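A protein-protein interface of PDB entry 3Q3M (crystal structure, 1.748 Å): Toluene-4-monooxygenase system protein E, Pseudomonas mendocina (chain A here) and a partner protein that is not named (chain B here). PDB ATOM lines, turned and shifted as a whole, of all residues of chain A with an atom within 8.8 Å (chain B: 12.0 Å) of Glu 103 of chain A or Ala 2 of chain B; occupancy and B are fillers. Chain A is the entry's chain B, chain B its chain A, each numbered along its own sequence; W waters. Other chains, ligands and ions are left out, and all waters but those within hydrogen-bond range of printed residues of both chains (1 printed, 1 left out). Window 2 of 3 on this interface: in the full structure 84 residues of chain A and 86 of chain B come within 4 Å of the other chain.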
ATOM      1  N   GLN A  95     -25.605  19.216  16.490  1.00  0.00           N
ATOM      2  CA  GLN A  95     -24.314  19.218  15.781  1.00  0.00           C
ATOM      3  C   GLN A  95     -24.478  19.602  14.305  1.00  0.00           C
ATOM      4  O   GLN A  95     -23.663  20.352  13.729  1.00  0.00           O
ATOM      5  CB  GLN A  95     -23.593  17.867  15.945  1.00  0.00           C
ATOM      6  CG  GLN A  95     -23.246  17.528  17.409  1.00  0.00           C
ATOM      7  CD  GLN A  95     -22.194  18.451  18.048  1.00  0.00           C
ATOM      8  OE1 GLN A  95     -21.099  18.616  17.515  1.00  0.00           O
ATOM      9  NE2 GLN A  95     -22.523  19.026  19.207  1.00  0.00           N
ATOM     10  N   SER A  96     -25.546  19.115  13.687  1.00  0.00           N
ATOM     11  CA  SER A  96     -25.846  19.511  12.312  1.00  0.00           C
ATOM     12  C   SER A  96     -26.186  21.000  12.178  1.00  0.00           C
ATOM     13  O   SER A  96     -25.876  21.609  11.160  1.00  0.00           O
ATOM     14  CB  SER A  96     -26.991  18.675  11.739  1.00  0.00           C
ATOM     15  OG  SER A  96     -26.556  17.354  11.461  1.00  0.00           O
ATOM     16  N   LEU A  97     -26.869  21.564  13.168  1.00  0.00           N
ATOM     17  CA  LEU A  97     -27.165  23.005  13.156  1.00  0.00           C
ATOM     18  C   LEU A  97     -25.857  23.777  13.244  1.00  0.00           C
ATOM     19  O   LEU A  97     -25.640  24.738  12.506  1.00  0.00           O
ATOM     20  CB  LEU A  97     -28.029  23.406  14.356  1.00  0.00           C
ATOM     21  CG  LEU A  97     -29.512  23.048  14.330  1.00  0.00           C
ATOM     22  CD1 LEU A  97     -30.100  23.335  15.713  1.00  0.00           C
ATOM     23  CD2 LEU A  97     -30.265  23.849  13.253  1.00  0.00           C
ATOM     24  N   PHE A  98     -25.001  23.378  14.174  1.00  0.00           N
ATOM     25  CA  PHE A  98     -23.705  24.044  14.318  1.00  0.00           C
ATOM     26  C   PHE A  98     -22.986  24.051  12.948  1.00  0.00           C
ATOM     27  O   PHE A  98     -22.491  25.088  12.508  1.00  0.00           O
ATOM     28  CB  PHE A  98     -22.823  23.323  15.345  1.00  0.00           C
ATOM     29  CG  PHE A  98     -23.256  23.483  16.786  1.00  0.00           C
ATOM     30  CD1 PHE A  98     -22.652  22.704  17.768  1.00  0.00           C
ATOM     31  CD2 PHE A  98     -24.220  24.416  17.167  1.00  0.00           C
ATOM     32  CE1 PHE A  98     -23.019  22.846  19.114  1.00  0.00           C
ATOM     33  CE2 PHE A  98     -24.588  24.555  18.477  1.00  0.00           C
ATOM     34  CZ  PHE A  98     -23.989  23.763  19.460  1.00  0.00           C
ATOM     35  N   ASP A  99     -22.941  22.895  12.288  1.00  0.00           N
ATOM     36  CA  ASP A  99     -22.218  22.725  11.009  1.00  0.00           C
ATOM     37  C   ASP A  99     -22.802  23.671   9.965  1.00  0.00           C
ATOM     38  O   ASP A  99     -22.072  24.418   9.290  1.00  0.00           O
ATOM     39  CB  ASP A  99     -22.354  21.273  10.538  1.00  0.00           C
ATOM     40  CG  ASP A  99     -21.477  20.944   9.320  1.00  0.00           C
ATOM     41  OD1 ASP A  99     -20.584  21.730   8.970  1.00  0.00           O
ATOM     42  OD2 ASP A  99     -21.690  19.871   8.721  1.00  0.00           O
ATOM     43  N   GLN A 100     -24.132  23.657   9.841  1.00  0.00           N
ATOM     44  CA  GLN A 100     -24.776  24.416   8.774  1.00  0.00           C
ATOM     45  C   GLN A 100     -24.725  25.911   9.061  1.00  0.00           C
ATOM     46  O   GLN A 100     -24.446  26.692   8.164  1.00  0.00           O
ATOM     47  CB  GLN A 100     -26.217  23.926   8.529  1.00  0.00           C
ATOM     48  CG  GLN A 100     -26.936  24.597   7.333  1.00  0.00           C
ATOM     49  CD  GLN A 100     -26.142  24.501   6.024  1.00  0.00           C
ATOM     50  OE1 GLN A 100     -25.587  23.456   5.687  1.00  0.00           O
ATOM     51  NE2 GLN A 100     -26.068  25.610   5.296  1.00  0.00           N
ATOM     52  N   PHE A 101     -24.993  26.318  10.303  1.00  0.00           N
ATOM     53  CA  PHE A 101     -24.935  27.736  10.628  1.00  0.00           C
ATOM     54  C   PHE A 101     -23.515  28.266  10.456  1.00  0.00           C
ATOM     55  O   PHE A 101     -23.295  29.425  10.039  1.00  0.00           O
ATOM     56  CB  PHE A 101     -25.494  28.002  12.039  1.00  0.00           C
ATOM     57  CG  PHE A 101     -26.989  28.069  12.068  1.00  0.00           C
ATOM     58  CD1 PHE A 101     -27.645  29.258  12.362  1.00  0.00           C
ATOM     59  CD2 PHE A 101     -27.749  26.963  11.714  1.00  0.00           C
ATOM     60  CE1 PHE A 101     -29.047  29.315  12.359  1.00  0.00           C
ATOM     61  CE2 PHE A 101     -29.143  27.020  11.697  1.00  0.00           C
ATOM     62  CZ  PHE A 101     -29.792  28.189  12.023  1.00  0.00           C
ATOM     63  N   ASN A 102     -22.542  27.412  10.734  1.00  0.00           N
ATOM     64  CA  ASN A 102     -21.150  27.792  10.508  1.00  0.00           C
ATOM     65  C   ASN A 102     -20.857  27.981   9.008  1.00  0.00           C
ATOM     66  O   ASN A 102     -20.205  28.945   8.603  1.00  0.00           O
ATOM     67  CB  ASN A 102     -20.180  26.780  11.127  1.00  0.00           C
ATOM     68  CG  ASN A 102     -18.741  27.019  10.678  1.00  0.00           C
ATOM     69  OD1 ASN A 102     -18.336  26.549   9.608  1.00  0.00           O
ATOM     70  ND2 ASN A 102     -17.968  27.784  11.482  1.00  0.00           N
ATOM     71  N   GLU A 103     -21.341  27.064   8.186  1.00  0.00           N
ATOM     72  CA  GLU A 103     -21.184  27.200   6.737  1.00  0.00           C
ATOM     73  C   GLU A 103     -21.745  28.523   6.244  1.00  0.00           C
ATOM     74  O   GLU A 103     -21.218  29.152   5.317  1.00  0.00           O
ATOM     75  CB  GLU A 103     -21.895  26.051   6.015  1.00  0.00           C
ATOM     76  CG  GLU A 103     -21.170  24.723   6.080  1.00  0.00           C
ATOM     77  CD  GLU A 103     -19.803  24.780   5.439  1.00  0.00           C
ATOM     78  OE1 GLU A 103     -18.823  24.354   6.080  1.00  0.00           O
ATOM     79  OE2 GLU A 103     -19.708  25.254   4.290  1.00  0.00           O
ATOM     80  N   ARG A 104     -22.854  28.929   6.850  1.00  0.00           N
ATOM     81  CA  ARG A 104     -23.557  30.125   6.438  1.00  0.00           C
ATOM     82  C   ARG A 104     -22.985  31.385   7.095  1.00  0.00           C
ATOM     83  O   ARG A 104     -23.504  32.488   6.904  1.00  0.00           O
ATOM     84  CB  ARG A 104     -25.055  29.960   6.726  1.00  0.00           C
ATOM     85  CG  ARG A 104     -25.744  29.019   5.746  1.00  0.00           C
ATOM     86  CD  ARG A 104     -25.512  29.515   4.309  1.00  0.00           C
ATOM     87  NE  ARG A 104     -26.230  28.734   3.301  1.00  0.00           N
ATOM     88  CZ  ARG A 104     -26.134  28.938   1.990  1.00  0.00           C
ATOM     89  NH1 ARG A 104     -25.348  29.898   1.516  1.00  0.00           N
ATOM     90  NH2 ARG A 104     -26.826  28.183   1.147  1.00  0.00           N
ATOM     91  N   GLU A 105     -21.905  31.220   7.864  1.00  0.00           N
ATOM     92  CA  GLU A 105     -21.254  32.347   8.523  1.00  0.00           C
ATOM     93  C   GLU A 105     -22.217  33.128   9.434  1.00  0.00           C
ATOM     94  O   GLU A 105     -22.176  34.381   9.522  1.00  0.00           O
ATOM     95  CB  GLU A 105     -20.580  33.260   7.475  1.00  0.00           C
ATOM     96  CG  GLU A 105     -19.428  32.570   6.721  1.00  0.00           C
ATOM     97  CD  GLU A 105     -18.937  33.352   5.502  1.00  0.00           C
ATOM     98  OE1 GLU A 105     -19.384  34.499   5.293  1.00  0.00           O
ATOM     99  OE2 GLU A 105     -18.104  32.817   4.740  1.00  0.00           O
ATOM    100  N   HIS A 106     -23.063  32.381  10.133  1.00  0.00           N
ATOM    101  CA  HIS A 106     -24.038  32.962  11.052  1.00  0.00           C
ATOM    102  C   HIS A 106     -23.439  33.983  12.023  1.00  0.00           C
ATOM    103  O   HIS A 106     -23.997  35.055  12.251  1.00  0.00           O
ATOM    104  CB  HIS A 106     -24.718  31.843  11.851  1.00  0.00           C
ATOM    105  CG  HIS A 106     -25.506  32.334  13.030  1.00  0.00           C
ATOM    106  ND1 HIS A 106     -24.934  32.576  14.263  1.00  0.00           N
ATOM    107  CD2 HIS A 106     -26.827  32.611  13.167  1.00  0.00           C
ATOM    108  CE1 HIS A 106     -25.866  32.992  15.105  1.00  0.00           C
ATOM    109  NE2 HIS A 106     -27.025  33.015  14.467  1.00  0.00           N
ATOM    110  N   ASP A 107     -22.309  33.646  12.625  1.00  0.00           N
ATOM    111  CA  ASP A 107     -21.759  34.499  13.666  1.00  0.00           C
ATOM    112  C   ASP A 107     -21.362  35.911  13.187  1.00  0.00           C
ATOM    113  O   ASP A 107     -21.378  36.857  13.975  1.00  0.00           O
ATOM    114  CB  ASP A 107     -20.595  33.798  14.365  1.00  0.00           C
ATOM    115  CG  ASP A 107     -21.043  32.593  15.160  1.00  0.00           C
ATOM    116  OD1 ASP A 107     -20.176  31.820  15.593  1.00  0.00           O
ATOM    117  OD2 ASP A 107     -22.266  32.406  15.339  1.00  0.00           O
ATOM    118  N   GLN A 108     -21.031  36.058  11.904  1.00  0.00           N
ATOM    119  CA  GLN A 108     -20.709  37.373  11.321  1.00  0.00           C
ATOM    120  C   GLN A 108     -21.886  38.345  11.215  1.00  0.00           C
ATOM    121  O   GLN A 108     -21.699  39.574  11.124  1.00  0.00           O
ATOM    122  CB  GLN A 108     -20.121  37.192   9.916  1.00  0.00           C
ATOM    123  CG  GLN A 108     -18.938  36.258   9.908  1.00  0.00           C
ATOM    124  CD  GLN A 108     -18.194  36.212   8.586  1.00  0.00           C
ATOM    125  OE1 GLN A 108     -18.285  37.135   7.765  1.00  0.00           O
ATOM    126  NE2 GLN A 108     -17.439  35.127   8.376  1.00  0.00           N
ATOM    127  N   TYR A 168     -18.173  24.504  23.228  1.00  0.00           N
ATOM    128  CA  TYR A 168     -18.032  24.472  21.782  1.00  0.00           C
ATOM    129  C   TYR A 168     -18.338  25.837  21.155  1.00  0.00           C
ATOM    130  O   TYR A 168     -17.601  26.331  20.297  1.00  0.00           O
ATOM    131  CB  TYR A 168     -18.956  23.412  21.162  1.00  0.00           C
ATOM    132  CG  TYR A 168     -18.763  23.292  19.658  1.00  0.00           C
ATOM    133  CD1 TYR A 168     -17.836  22.386  19.128  1.00  0.00           C
ATOM    134  CD2 TYR A 168     -19.470  24.103  18.766  1.00  0.00           C
ATOM    135  CE1 TYR A 168     -17.637  22.261  17.760  1.00  0.00           C
ATOM    136  CE2 TYR A 168     -19.262  24.000  17.383  1.00  0.00           C
ATOM    137  CZ  TYR A 168     -18.337  23.071  16.896  1.00  0.00           C
ATOM    138  OH  TYR A 168     -18.106  22.902  15.549  1.00  0.00           O
ATOM    139  N   ARG A 169     -19.438  26.443  21.588  1.00  0.00           N
ATOM    140  CA  ARG A 169     -19.875  27.702  21.004  1.00  0.00           C
ATOM    141  C   ARG A 169     -19.011  28.888  21.457  1.00  0.00           C
ATOM    142  O   ARG A 169     -18.826  29.844  20.718  1.00  0.00           O
ATOM    143  CB  ARG A 169     -21.353  27.940  21.283  1.00  0.00           C
ATOM    144  CG  ARG A 169     -22.255  27.098  20.376  1.00  0.00           C
ATOM    145  CD  ARG A 169     -22.252  27.578  18.921  1.00  0.00           C
ATOM    146  NE  ARG A 169     -22.716  28.961  18.843  1.00  0.00           N
ATOM    147  CZ  ARG A 169     -22.267  29.847  17.965  1.00  0.00           C
ATOM    148  NH1 ARG A 169     -22.732  31.087  18.002  1.00  0.00           N
ATOM    149  NH2 ARG A 169     -21.329  29.503  17.079  1.00  0.00           N
ATOM    150  N   GLU A 172     -16.080  28.501  19.197  1.00  0.00           N
ATOM    151  CA  GLU A 172     -16.476  28.876  17.844  1.00  0.00           C
ATOM    152  C   GLU A 172     -16.652  30.389  17.667  1.00  0.00           C
ATOM    153  O   GLU A 172     -16.145  30.974  16.708  1.00  0.00           O
ATOM    154  CB  GLU A 172     -17.739  28.132  17.402  1.00  0.00           C
ATOM    155  CG  GLU A 172     -18.137  28.482  15.960  1.00  0.00           C
ATOM    156  CD  GLU A 172     -19.105  27.494  15.368  1.00  0.00           C
ATOM    157  OE1 GLU A 172     -18.851  26.989  14.254  1.00  0.00           O
ATOM    158  OE2 GLU A 172     -20.134  27.232  16.011  1.00  0.00           O
ATOM    159  N   LEU A 175     -13.593  32.573  17.183  1.00  0.00           N
ATOM    160  CA  LEU A 175     -12.952  32.555  15.867  1.00  0.00           C
ATOM    161  C   LEU A 175     -13.354  33.753  15.023  1.00  0.00           C
ATOM    162  O   LEU A 175     -12.527  34.319  14.285  1.00  0.00           O
ATOM    163  CB  LEU A 175     -13.305  31.258  15.123  1.00  0.00           C
ATOM    164  CG  LEU A 175     -12.839  29.974  15.815  1.00  0.00           C
ATOM    165  CD1 LEU A 175     -13.250  28.779  15.004  1.00  0.00           C
ATOM    166  CD2 LEU A 175     -11.317  29.963  16.053  1.00  0.00           C
ATOM    167  N   ALA B   2     -18.951  23.955   8.649  1.00  0.00           N
ATOM    168  CA  ALA B   2     -17.846  23.127   9.128  1.00  0.00           C
ATOM    169  C   ALA B   2     -17.931  22.894  10.639  1.00  0.00           C
ATOM    170  O   ALA B   2     -18.610  23.653  11.362  1.00  0.00           O
ATOM    171  CB  ALA B   2     -16.518  23.790   8.771  1.00  0.00           C
ATOM    172  N   MET B   3     -17.220  21.872  11.109  1.00  0.00           N
ATOM    173  CA  MET B   3     -17.137  21.544  12.543  1.00  0.00           C
ATOM    174  C   MET B   3     -15.697  21.764  12.993  1.00  0.00           C
ATOM    175  O   MET B   3     -14.754  21.606  12.196  1.00  0.00           O
ATOM    176  CB  MET B   3     -17.500  20.083  12.799  1.00  0.00           C
ATOM    177  CG  MET B   3     -18.926  19.673  12.402  1.00  0.00           C
ATOM    178  SD  MET B   3     -20.137  20.659  13.278  1.00  0.00           S
ATOM    179  CE  MET B   3     -19.913  20.072  14.961  1.00  0.00           C
ATOM    180  N   HIS B   4     -15.518  22.117  14.261  1.00  0.00           N
ATOM    181  CA  HIS B   4     -14.180  22.362  14.799  1.00  0.00           C
ATOM    182  C   HIS B   4     -13.744  21.153  15.612  1.00  0.00           C
ATOM    183  O   HIS B   4     -14.520  20.632  16.402  1.00  0.00           O
ATOM    184  CB  HIS B   4     -14.204  23.637  15.639  1.00  0.00           C
ATOM    185  CG  HIS B   4     -14.845  24.782  14.916  1.00  0.00           C
ATOM    186  ND1 HIS B   4     -14.275  25.364  13.808  1.00  0.00           N
ATOM    187  CD2 HIS B   4     -16.041  25.396  15.092  1.00  0.00           C
ATOM    188  CE1 HIS B   4     -15.080  26.306  13.344  1.00  0.00           C
ATOM    189  NE2 HIS B   4     -16.161  26.341  14.103  1.00  0.00           N
ATOM    190  N   PRO B   5     -12.501  20.690  15.401  1.00  0.00           N
ATOM    191  CA  PRO B   5     -12.056  19.447  16.032  1.00  0.00           C
ATOM    192  C   PRO B   5     -11.956  19.559  17.547  1.00  0.00           C
ATOM    193  O   PRO B   5     -11.626  20.620  18.092  1.00  0.00           O
ATOM    194  CB  PRO B   5     -10.659  19.234  15.437  1.00  0.00           C
ATOM    195  CG  PRO B   5     -10.205  20.566  15.006  1.00  0.00           C
ATOM    196  CD  PRO B   5     -11.448  21.302  14.572  1.00  0.00           C
ATOM    197  N   ARG B   6     -12.220  18.447  18.218  1.00  0.00           N
ATOM    198  CA  ARG B   6     -12.245  18.428  19.677  1.00  0.00           C
ATOM    199  C   ARG B   6     -11.015  19.060  20.334  1.00  0.00           C
ATOM    200  O   ARG B   6     -11.151  19.748  21.333  1.00  0.00           O
ATOM    201  CB  ARG B   6     -12.419  17.003  20.187  1.00  0.00           C
ATOM    202  CG  ARG B   6     -12.799  16.959  21.684  1.00  0.00           C
ATOM    203  CD  ARG B   6     -13.122  15.534  22.081  1.00  0.00           C
ATOM    204  NE  ARG B   6     -11.904  14.738  22.133  1.00  0.00           N
ATOM    205  CZ  ARG B   6     -11.872  13.415  22.003  1.00  0.00           C
ATOM    206  NH1 ARG B   6     -12.998  12.741  21.777  1.00  0.00           N
ATOM    207  NH2 ARG B   6     -10.710  12.779  22.067  1.00  0.00           N
ATOM    208  N   ASP B   8      -9.415  21.575  19.788  1.00  0.00           N
ATOM    209  CA  ASP B   8      -9.470  23.033  19.856  1.00  0.00           C
ATOM    210  C   ASP B   8     -10.434  23.590  20.912  1.00  0.00           C
ATOM    211  O   ASP B   8     -10.314  24.771  21.293  1.00  0.00           O
ATOM    212  CB  ASP B   8      -9.840  23.623  18.497  1.00  0.00           C
ATOM    213  CG  ASP B   8      -8.842  23.270  17.410  1.00  0.00           C
ATOM    214  OD1 ASP B   8      -7.775  22.700  17.718  1.00  0.00           O
ATOM    215  OD2 ASP B   8      -9.135  23.579  16.256  1.00  0.00           O
ATOM    216  N   TRP B   9     -11.379  22.776  21.379  1.00  0.00           N
ATOM    217  CA  TRP B   9     -12.319  23.247  22.401  1.00  0.00           C
ATOM    218  C   TRP B   9     -12.367  22.397  23.656  1.00  0.00           C
ATOM    219  O   TRP B   9     -13.057  22.766  24.609  1.00  0.00           O
ATOM    220  CB  TRP B   9     -13.742  23.440  21.839  1.00  0.00           C
ATOM    221  CG  TRP B   9     -14.241  22.253  21.016  1.00  0.00           C
ATOM    222  CD1 TRP B   9     -14.153  22.110  19.666  1.00  0.00           C
ATOM    223  CD2 TRP B   9     -14.892  21.069  21.504  1.00  0.00           C
ATOM    224  NE1 TRP B   9     -14.702  20.912  19.277  1.00  0.00           N
ATOM    225  CE2 TRP B   9     -15.168  20.254  20.382  1.00  0.00           C
ATOM    226  CE3 TRP B   9     -15.270  20.614  22.782  1.00  0.00           C
ATOM    227  CZ2 TRP B   9     -15.787  19.009  20.491  1.00  0.00           C
ATOM    228  CZ3 TRP B   9     -15.891  19.369  22.885  1.00  0.00           C
ATOM    229  CH2 TRP B   9     -16.136  18.581  21.744  1.00  0.00           C
HETATM  230  O   HOH W   1     -22.039  17.884  12.438  1.00  0.00           O
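The backbone NH (N) of Ala 2 of chain B sits at hydrogen-bond distance from the side-chain carboxylate (OD1) of Asp 99 of chain A (2.8 Å). N of Ala 2 of chain B sits at hydrogen-bond distance from OD1 of Asn 102 of chain A, at 2.8 Å. The side-chain carboxylate (OE1) of Glu 103 of chain A is in hydrogen-bond range of the backbone NH (N) of Ala 2 of chain B, 2.6 Å away. The backbone NH of Asp 99 of chain A lies close to the side-chain sulfur of Met 3 of chain B (3.7 Å). SD of Met 3 of chain B sits close to OH of Tyr 168 of chain A, 3.8 Å away. A ring nitrogen (NE2) of His 4 of chain B sits at hydrogen-bond distance from the side-chain amide nitrogen of Asn 102 of chain A. The backbone NH of His 4 of chain B is in hydrogen-bond range of the side-chain hydroxyl of Tyr 168 of chain A, 3.0 Å away. OE1 of Glu 172 of chain A sits at hydrogen-bond distance from NE2 of His 4 of chain B (2.8 Å). The backbone carbonyl oxygen (O) of Gln 95 of chain A lies close to the side-chain sulfur (SD) of Met 3 of chain B.
The indole nitrogen (NE1) of Trp 9 of chain B sits at hydrogen-bond distance from the backbone carbonyl oxygen (O) of His 4 of chain B (2.9 Å). The backbone carbonyl oxygen (O) of Pro 5 of chain B sits at hydrogen-bond distance from the indole nitrogen (NE1) of Trp 9 of chain B, 3.3 Å away. ND2 of Asn 102 of chain A lies within hydrogen-bond range of OE1 of Glu 172 of chain A, at 3.0 Å. NH2 of Arg 169 of chain A is in salt-bridge range of OE2 of Glu 172 of chain A (2.8 Å).
Tyr 168 of chain A touches Trp 9 of chain B. CE1 of His 4 of chain B touches CD1 of Leu 175 of chain A, 3.5 Å away.
Of the printed residues of chain B, Gln 95 of chain A touches Met 3 (3.2 Å). Of chain B, only Ala 2 (2.8 Å) and Met 3 (3.6 Å) come within 4 Å of Asp 99 of chain A. Of chain B, only Ala 2 (2.6 Å) comes within 4 Å of Glu 103 of chain A. No residue of chain B comes within 4 Å of Arg 104 of chain A. No residue of chain B comes within 4 Å of Glu 105 of chain A. Ala 2 of chain B touches just these residues of chain A: Asp 99 (2.8 Å), Asn 102 (2.8 Å) and Glu 103 (2.6 Å). Printed residues of chain A within 4 Å of Met 3 of chain B: Gln 95, Asp 99 and Tyr 168. The nearest printed residue of chain B that does not touch Glu 172 of chain A is Ala 2 of chain B (4.4 Å).
Of the 18 printed residues of chain A, 7 touch a printed residue of chain B. Printed residues of chain A that touch a printed residue of chain B: Gln 95, Asp 99, Asn 102, Glu 103, Tyr 168, Glu 172 and Leu 175. Hydrophobic or aromatic side chains of chain A within 4 Å of the printed part of chain B: Tyr 168 and Leu 175. Among the printed residues, no Asp or Glu carboxylate lies within 4 Å of a Lys or Arg side-chain nitrogen of the other chain.
Water W1 lies within hydrogen-bond range of the backbone carbonyl oxygen of Gln 95 of chain A (3.2 Å) and the side-chain sulfur of Met 3 of chain B (3.5 Å).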
